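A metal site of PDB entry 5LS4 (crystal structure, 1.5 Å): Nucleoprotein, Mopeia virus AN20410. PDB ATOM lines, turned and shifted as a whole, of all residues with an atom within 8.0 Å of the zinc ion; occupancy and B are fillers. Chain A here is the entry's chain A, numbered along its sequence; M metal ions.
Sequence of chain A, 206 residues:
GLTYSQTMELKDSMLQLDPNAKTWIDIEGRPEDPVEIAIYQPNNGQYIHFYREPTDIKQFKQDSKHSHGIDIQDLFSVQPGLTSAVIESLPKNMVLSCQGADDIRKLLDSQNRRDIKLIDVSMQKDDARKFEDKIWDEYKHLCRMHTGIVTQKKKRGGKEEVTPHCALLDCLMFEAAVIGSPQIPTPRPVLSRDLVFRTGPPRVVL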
ATOM      1  N   GLU A  28      14.804  -1.658 -19.388  1.00  0.00           N
ATOM      2  CA  GLU A  28      13.821  -2.214 -18.479  1.00  0.00           C
ATOM      3  C   GLU A  28      13.943  -3.731 -18.503  1.00  0.00           C
ATOM      4  O   GLU A  28      14.307  -4.328 -19.537  1.00  0.00           O
ATOM      5  CB  GLU A  28      12.408  -1.766 -18.815  1.00  0.00           C
ATOM      6  CG  GLU A  28      12.215  -0.274 -18.554  1.00  0.00           C
ATOM      7  CD  GLU A  28      12.229   0.052 -17.049  1.00  0.00           C
ATOM      8  OE1 GLU A  28      11.674  -0.760 -16.267  1.00  0.00           O
ATOM      9  OE2 GLU A  28      12.761   1.120 -16.688  1.00  0.00           O
ATOM     10  N   VAL A  35      13.841  -6.499 -21.303  1.00  0.00           N
ATOM     11  CA  VAL A  35      12.684  -6.478 -22.193  1.00  0.00           C
ATOM     12  C   VAL A  35      12.576  -5.194 -23.034  1.00  0.00           C
ATOM     13  O   VAL A  35      11.808  -5.163 -23.998  1.00  0.00           O
ATOM     14  CB  VAL A  35      11.361  -6.719 -21.426  1.00  0.00           C
ATOM     15  CG1 VAL A  35      11.381  -8.103 -20.771  1.00  0.00           C
ATOM     16  CG2 VAL A  35      11.115  -5.617 -20.392  1.00  0.00           C
ATOM     17  N   GLU A  36      13.354  -4.155 -22.703  1.00  0.00           N
ATOM     18  CA  GLU A  36      13.303  -2.894 -23.447  1.00  0.00           C
ATOM     19  C   GLU A  36      14.625  -2.181 -23.297  1.00  0.00           C
ATOM     20  O   GLU A  36      15.152  -2.088 -22.181  1.00  0.00           O
ATOM     21  CB  GLU A  36      12.185  -1.979 -22.951  1.00  0.00           C
ATOM     22  CG  GLU A  36      11.909  -0.760 -23.861  1.00  0.00           C
ATOM     23  CD  GLU A  36      10.865   0.185 -23.332  1.00  0.00           C
ATOM     24  OE1 GLU A  36      10.672   0.287 -22.095  1.00  0.00           O
ATOM     25  OE2 GLU A  36      10.194   0.822 -24.171  1.00  0.00           O
ATOM     26  N   ILE A  37      15.188  -1.736 -24.417  1.00  0.00           N
ATOM     27  CA  ILE A  37      16.497  -1.048 -24.421  1.00  0.00           C
ATOM     28  C   ILE A  37      16.405   0.211 -25.261  1.00  0.00           C
ATOM     29  O   ILE A  37      15.807   0.180 -26.346  1.00  0.00           O
ATOM     30  CB  ILE A  37      17.583  -1.990 -25.000  1.00  0.00           C
ATOM     31  CG1 ILE A  37      17.716  -3.228 -24.097  1.00  0.00           C
ATOM     32  CG2 ILE A  37      18.914  -1.259 -25.187  1.00  0.00           C
ATOM     33  CD1 ILE A  37      18.727  -4.241 -24.538  1.00  0.00           C
ATOM     34  N   ALA A  38      16.984   1.311 -24.759  1.00  0.00           N
ATOM     35  CA  ALA A  38      17.096   2.552 -25.508  1.00  0.00           C
ATOM     36  C   ALA A  38      18.504   3.111 -25.396  1.00  0.00           C
ATOM     37  O   ALA A  38      19.097   3.087 -24.329  1.00  0.00           O
ATOM     38  CB  ALA A  38      16.052   3.577 -25.045  1.00  0.00           C
ATOM     39  N   HIS A  49      16.020   1.897 -30.297  1.00  0.00           N
ATOM     40  CA  HIS A  49      15.051   1.493 -29.277  1.00  0.00           C
ATOM     41  C   HIS A  49      14.357   0.247 -29.751  1.00  0.00           C
ATOM     42  O   HIS A  49      13.879   0.182 -30.898  1.00  0.00           O
ATOM     43  CB  HIS A  49      14.050   2.629 -29.060  1.00  0.00           C
ATOM     44  CG  HIS A  49      12.907   2.311 -28.149  1.00  0.00           C
ATOM     45  ND1 HIS A  49      11.621   2.671 -28.461  1.00  0.00           N
ATOM     46  CD2 HIS A  49      12.834   1.724 -26.919  1.00  0.00           C
ATOM     47  CE1 HIS A  49      10.798   2.319 -27.481  1.00  0.00           C
ATOM     48  NE2 HIS A  49      11.509   1.729 -26.548  1.00  0.00           N
ATOM     49  N   PHE A  50      14.268  -0.750 -28.881  1.00  0.00           N
ATOM     50  CA  PHE A  50      13.655  -2.046 -29.252  1.00  0.00           C
ATOM     51  C   PHE A  50      13.302  -2.821 -27.998  1.00  0.00           C
ATOM     52  O   PHE A  50      13.606  -2.387 -26.884  1.00  0.00           O
ATOM     53  CB  PHE A  50      14.582  -2.867 -30.158  1.00  0.00           C
ATOM     54  CG  PHE A  50      15.915  -3.146 -29.537  1.00  0.00           C
ATOM     55  CD1 PHE A  50      16.935  -2.226 -29.627  1.00  0.00           C
ATOM     56  CD2 PHE A  50      16.128  -4.289 -28.810  1.00  0.00           C
ATOM     57  CE1 PHE A  50      18.156  -2.462 -29.038  1.00  0.00           C
ATOM     58  CE2 PHE A  50      17.337  -4.531 -28.203  1.00  0.00           C
ATOM     59  CZ  PHE A  50      18.362  -3.630 -28.331  1.00  0.00           C
ATOM     60  N   TYR A  51      12.656  -3.973 -28.220  1.00  0.00           N
ATOM     61  CA  TYR A  51      12.088  -4.797 -27.153  1.00  0.00           C
ATOM     62  C   TYR A  51      12.583  -6.235 -27.252  1.00  0.00           C
ATOM     63  O   TYR A  51      13.150  -6.631 -28.273  1.00  0.00           O
ATOM     64  CB  TYR A  51      10.557  -4.799 -27.255  1.00  0.00           C
ATOM     65  CG  TYR A  51       9.977  -3.419 -27.471  1.00  0.00           C
ATOM     66  CD1 TYR A  51       9.722  -2.557 -26.413  1.00  0.00           C
ATOM     67  CD2 TYR A  51       9.694  -2.981 -28.753  1.00  0.00           C
ATOM     68  CE1 TYR A  51       9.199  -1.283 -26.636  1.00  0.00           C
ATOM     69  CE2 TYR A  51       9.150  -1.737 -28.995  1.00  0.00           C
ATOM     70  CZ  TYR A  51       8.915  -0.894 -27.941  1.00  0.00           C
ATOM     71  OH  TYR A  51       8.369   0.376 -28.209  1.00  0.00           O
ATOM     72  N   HIS A  68       7.474  -1.341 -15.382  1.00  0.00           N
ATOM     73  CA  HIS A  68       7.267  -0.901 -16.775  1.00  0.00           C
ATOM     74  C   HIS A  68       5.843  -1.022 -17.351  1.00  0.00           C
ATOM     75  O   HIS A  68       5.553  -0.414 -18.371  1.00  0.00           O
ATOM     76  CB  HIS A  68       8.281  -1.584 -17.724  1.00  0.00           C
ATOM     77  CG  HIS A  68       8.279  -3.075 -17.664  1.00  0.00           C
ATOM     78  ND1 HIS A  68       7.184  -3.848 -17.993  1.00  0.00           N
ATOM     79  CD2 HIS A  68       9.255  -3.939 -17.307  1.00  0.00           C
ATOM     80  CE1 HIS A  68       7.488  -5.124 -17.845  1.00  0.00           C
ATOM     81  NE2 HIS A  68       8.749  -5.211 -17.439  1.00  0.00           N
ATOM     82  N   ILE A  70       4.391  -3.222 -19.064  1.00  0.00           N
ATOM     83  CA  ILE A  70       4.232  -3.895 -20.360  1.00  0.00           C
ATOM     84  C   ILE A  70       3.443  -5.199 -20.221  1.00  0.00           C
ATOM     85  O   ILE A  70       3.670  -5.993 -19.306  1.00  0.00           O
ATOM     86  CB  ILE A  70       5.597  -4.176 -21.021  1.00  0.00           C
ATOM     87  CG1 ILE A  70       6.393  -2.872 -21.173  1.00  0.00           C
ATOM     88  CG2 ILE A  70       5.406  -4.828 -22.376  1.00  0.00           C
ATOM     89  CD1 ILE A  70       7.857  -3.066 -21.633  1.00  0.00           C
ATOM     90  N   TRP A 136       6.138  12.677 -21.149  1.00  0.00           N
ATOM     91  CA  TRP A 136       5.012  11.867 -21.608  1.00  0.00           C
ATOM     92  C   TRP A 136       3.999  12.664 -22.431  1.00  0.00           C
ATOM     93  O   TRP A 136       3.508  12.158 -23.439  1.00  0.00           O
ATOM     94  CB  TRP A 136       4.318  11.146 -20.435  1.00  0.00           C
ATOM     95  CG  TRP A 136       5.079   9.924 -20.022  1.00  0.00           C
ATOM     96  CD1 TRP A 136       6.033   9.847 -19.074  1.00  0.00           C
ATOM     97  CD2 TRP A 136       4.951   8.598 -20.573  1.00  0.00           C
ATOM     98  NE1 TRP A 136       6.539   8.562 -18.992  1.00  0.00           N
ATOM     99  CE2 TRP A 136       5.880   7.784 -19.902  1.00  0.00           C
ATOM    100  CE3 TRP A 136       4.150   8.036 -21.584  1.00  0.00           C
ATOM    101  CZ2 TRP A 136       6.028   6.427 -20.183  1.00  0.00           C
ATOM    102  CZ3 TRP A 136       4.308   6.670 -21.867  1.00  0.00           C
ATOM    103  CH2 TRP A 136       5.232   5.898 -21.167  1.00  0.00           C
ATOM    104  N   LYS A 140       4.671  10.595 -25.807  1.00  0.00           N
ATOM    105  CA  LYS A 140       3.949   9.343 -25.614  1.00  0.00           C
ATOM    106  C   LYS A 140       3.790   8.533 -26.916  1.00  0.00           C
ATOM    107  O   LYS A 140       3.714   7.309 -26.886  1.00  0.00           O
ATOM    108  CB  LYS A 140       2.559   9.583 -24.991  1.00  0.00           C
ATOM    109  CG  LYS A 140       1.601  10.335 -25.913  1.00  0.00           C
ATOM    110  CD  LYS A 140       0.425  10.938 -25.176  1.00  0.00           C
ATOM    111  CE  LYS A 140      -0.357  11.883 -26.083  1.00  0.00           C
ATOM    112  NZ  LYS A 140      -1.411  12.613 -25.352  1.00  0.00           N
ATOM    113  N   LEU A 142       5.874   7.951 -29.130  1.00  0.00           N
ATOM    114  CA  LEU A 142       7.084   7.206 -29.496  1.00  0.00           C
ATOM    115  C   LEU A 142       7.163   5.799 -28.872  1.00  0.00           C
ATOM    116  O   LEU A 142       7.959   4.986 -29.317  1.00  0.00           O
ATOM    117  CB  LEU A 142       8.330   8.005 -29.107  1.00  0.00           C
ATOM    118  CG  LEU A 142       8.504   9.388 -29.750  1.00  0.00           C
ATOM    119  CD1 LEU A 142       9.809  10.040 -29.268  1.00  0.00           C
ATOM    120  CD2 LEU A 142       8.482   9.290 -31.255  1.00  0.00           C
ATOM    121  N   CYS A 143       6.367   5.530 -27.839  1.00  0.00           N
ATOM    122  CA  CYS A 143       6.305   4.176 -27.295  1.00  0.00           C
ATOM    123  C   CYS A 143       4.955   3.937 -26.625  1.00  0.00           C
ATOM    124  O   CYS A 143       4.638   4.524 -25.596  1.00  0.00           O
ATOM    125  CB  CYS A 143       7.435   3.932 -26.302  1.00  0.00           C
ATOM    126  SG  CYS A 143       7.465   2.186 -25.757  1.00  0.00           S
ATOM    127  N   ARG A 144       4.181   3.010 -27.199  1.00  0.00           N
ATOM    128  CA  ARG A 144       2.820   2.778 -26.713  1.00  0.00           C
ATOM    129  C   ARG A 144       2.716   1.448 -25.959  1.00  0.00           C
ATOM    130  O   ARG A 144       1.619   0.938 -25.741  1.00  0.00           O
ATOM    131  CB  ARG A 144       1.814   2.801 -27.868  1.00  0.00           C
ATOM    132  CG  ARG A 144       1.733   4.142 -28.540  1.00  0.00           C
ATOM    133  CD  ARG A 144       0.510   4.228 -29.429  1.00  0.00           C
ATOM    134  NE  ARG A 144       0.265   5.601 -29.861  1.00  0.00           N
ATOM    135  CZ  ARG A 144       0.788   6.148 -30.965  1.00  0.00           C
ATOM    136  NH1 ARG A 144       1.597   5.433 -31.737  1.00  0.00           N
ATOM    137  NH2 ARG A 144       0.503   7.409 -31.280  1.00  0.00           N
ATOM    138  N   MET A 145       3.859   0.899 -25.554  1.00  0.00           N
ATOM    139  CA  MET A 145       3.905  -0.408 -24.926  1.00  0.00           C
ATOM    140  C   MET A 145       3.586  -0.502 -23.439  1.00  0.00           C
ATOM    141  O   MET A 145       3.521  -1.620 -22.918  1.00  0.00           O
ATOM    142  CB  MET A 145       5.279  -0.999 -25.153  1.00  0.00           C
ATOM    143  CG  MET A 145       5.601  -1.208 -26.608  1.00  0.00           C
ATOM    144  SD  MET A 145       4.722  -2.605 -27.331  1.00  0.00           S
ATOM    145  CE  MET A 145       5.508  -3.884 -26.431  1.00  0.00           C
ATOM    146  N   HIS A 146       3.379   0.637 -22.765  1.00  0.00           N
ATOM    147  CA  HIS A 146       3.234   0.669 -21.312  1.00  0.00           C
ATOM    148  C   HIS A 146       1.779   0.868 -20.928  1.00  0.00           C
ATOM    149  O   HIS A 146       1.358   1.957 -20.570  1.00  0.00           O
ATOM    150  CB  HIS A 146       4.159   1.745 -20.744  1.00  0.00           C
ATOM    151  CG  HIS A 146       5.566   1.588 -21.230  1.00  0.00           C
ATOM    152  ND1 HIS A 146       6.494   0.820 -20.576  1.00  0.00           N
ATOM    153  CD2 HIS A 146       6.171   2.040 -22.358  1.00  0.00           C
ATOM    154  CE1 HIS A 146       7.616   0.799 -21.265  1.00  0.00           C
ATOM    155  NE2 HIS A 146       7.458   1.544 -22.344  1.00  0.00           N
ATOM    156  N   PRO A 164       4.343   4.562 -15.616  1.00  0.00           N
ATOM    157  CA  PRO A 164       5.228   3.444 -15.971  1.00  0.00           C
ATOM    158  C   PRO A 164       6.588   3.905 -16.486  1.00  0.00           C
ATOM    159  O   PRO A 164       6.716   4.980 -17.076  1.00  0.00           O
ATOM    160  CB  PRO A 164       4.447   2.721 -17.074  1.00  0.00           C
ATOM    161  CG  PRO A 164       3.024   3.097 -16.846  1.00  0.00           C
ATOM    162  CD  PRO A 164       3.050   4.500 -16.329  1.00  0.00           C
ATOM    163  N   HIS A 165       7.593   3.067 -16.292  1.00  0.00           N
ATOM    164  CA  HIS A 165       8.936   3.359 -16.757  1.00  0.00           C
ATOM    165  C   HIS A 165       9.173   2.783 -18.139  1.00  0.00           C
ATOM    166  O   HIS A 165       9.011   1.583 -18.362  1.00  0.00           O
ATOM    167  CB  HIS A 165       9.967   2.825 -15.774  1.00  0.00           C
ATOM    168  CG  HIS A 165       9.904   3.498 -14.440  1.00  0.00           C
ATOM    169  ND1 HIS A 165      10.695   3.118 -13.377  1.00  0.00           N
ATOM    170  CD2 HIS A 165       9.139   4.515 -13.991  1.00  0.00           C
ATOM    171  CE1 HIS A 165      10.420   3.876 -12.336  1.00  0.00           C
ATOM    172  NE2 HIS A 165       9.478   4.731 -12.674  1.00  0.00           N
ATOM    173  N   CYS A 166       9.527   3.668 -19.053  1.00  0.00           N
ATOM    174  CA  CYS A 166       9.864   3.354 -20.440  1.00  0.00           C
ATOM    175  C   CYS A 166      11.340   3.663 -20.652  1.00  0.00           C
ATOM    176  O   CYS A 166      11.802   4.757 -20.322  1.00  0.00           O
ATOM    177  CB  CYS A 166       9.012   4.189 -21.402  1.00  0.00           C
ATOM    178  SG  CYS A 166       9.550   4.215 -23.121  1.00  0.00           S
ATOM    179  N   ALA A 167      12.104   2.708 -21.193  1.00  0.00           N
ATOM    180  CA  ALA A 167      13.551   2.926 -21.378  1.00  0.00           C
ATOM    181  C   ALA A 167      13.822   4.186 -22.231  1.00  0.00           C
ATOM    182  O   ALA A 167      14.774   4.932 -21.975  1.00  0.00           O
ATOM    183  CB  ALA A 167      14.180   1.728 -22.031  1.00  0.00           C
ATOM    184  N   LEU A 168      13.008   4.393 -23.256  1.00  0.00           N
ATOM    185  CA  LEU A 168      13.206   5.530 -24.165  1.00  0.00           C
ATOM    186  C   LEU A 168      12.851   6.846 -23.481  1.00  0.00           C
ATOM    187  O   LEU A 168      13.672   7.764 -23.408  1.00  0.00           O
ATOM    188  CB  LEU A 168      12.400   5.356 -25.455  1.00  0.00           C
ATOM    189  CG  LEU A 168      12.501   6.581 -26.380  1.00  0.00           C
ATOM    190  CD1 LEU A 168      13.926   6.796 -26.902  1.00  0.00           C
ATOM    191  CD2 LEU A 168      11.523   6.363 -27.514  1.00  0.00           C
ATOM    192  N   LEU A 169      11.640   6.938 -22.933  1.00  0.00           N
ATOM    193  CA  LEU A 169      11.228   8.194 -22.320  1.00  0.00           C
ATOM    194  C   LEU A 169      12.026   8.504 -21.054  1.00  0.00           C
ATOM    195  O   LEU A 169      12.225   9.670 -20.728  1.00  0.00           O
ATOM    196  CB  LEU A 169       9.714   8.212 -22.088  1.00  0.00           C
ATOM    197  CG  LEU A 169       8.899   8.785 -23.267  1.00  0.00           C
ATOM    198  CD1 LEU A 169       9.096   8.004 -24.554  1.00  0.00           C
ATOM    199  CD2 LEU A 169       7.429   8.872 -22.890  1.00  0.00           C
ATOM    200  N   ASP A 170      12.534   7.476 -20.374  1.00  0.00           N
ATOM    201  CA  ASP A 170      13.463   7.702 -19.275  1.00  0.00           C
ATOM    202  C   ASP A 170      14.720   8.410 -19.780  1.00  0.00           C
ATOM    203  O   ASP A 170      15.142   9.413 -19.195  1.00  0.00           O
ATOM    204  CB  ASP A 170      13.828   6.389 -18.565  1.00  0.00           C
ATOM    205  CG  ASP A 170      12.770   5.936 -17.578  1.00  0.00           C
ATOM    206  OD1 ASP A 170      11.736   6.613 -17.428  1.00  0.00           O
ATOM    207  OD2 ASP A 170      13.002   4.884 -16.923  1.00  0.00           O
HETATM  208 ZN    ZN M   1       8.762   2.177 -23.820  1.00  0.00          ZN
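The side-chain sulfur of Cys 166 sits close to the backbone NH of Leu 168, at 3.5 Å.
The side-chain sulfur of Cys 166 sits close to the backbone NH of Leu 169 (3.4 Å).
ND1 of His 146 sits close to O of His 165.
The backbone carbonyl oxygen (O) of Glu 36 is in hydrogen-bond range of the backbone NH (N) of Glu 28.
ND1 of His 146 is in hydrogen-bond range of O of His 68 (2.7 Å).
SG of Cys 143 sits close to OH of Tyr 51 (3.2 Å).
A ring nitrogen (NE2) of His 49 lies close to the side-chain carboxylate (OE2) of Glu 36, at 2.9 Å.
The side-chain carboxylate (OE1) of Glu 36 sits at hydrogen-bond distance from the backbone NH (N) of Ala 167, at 3.0 Å.
Merely in contact with the zinc ion: His 49 (3.9 Å).
The zinc ion is bound by OE2 of Glu 36 (2.0 Å), NE2 of His 146 (2.1 Å), SG of Cys 166 (2.3 Å) and SG of Cys 143 (2.3 Å).
The zinc ion has four donor atoms within binding distance.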
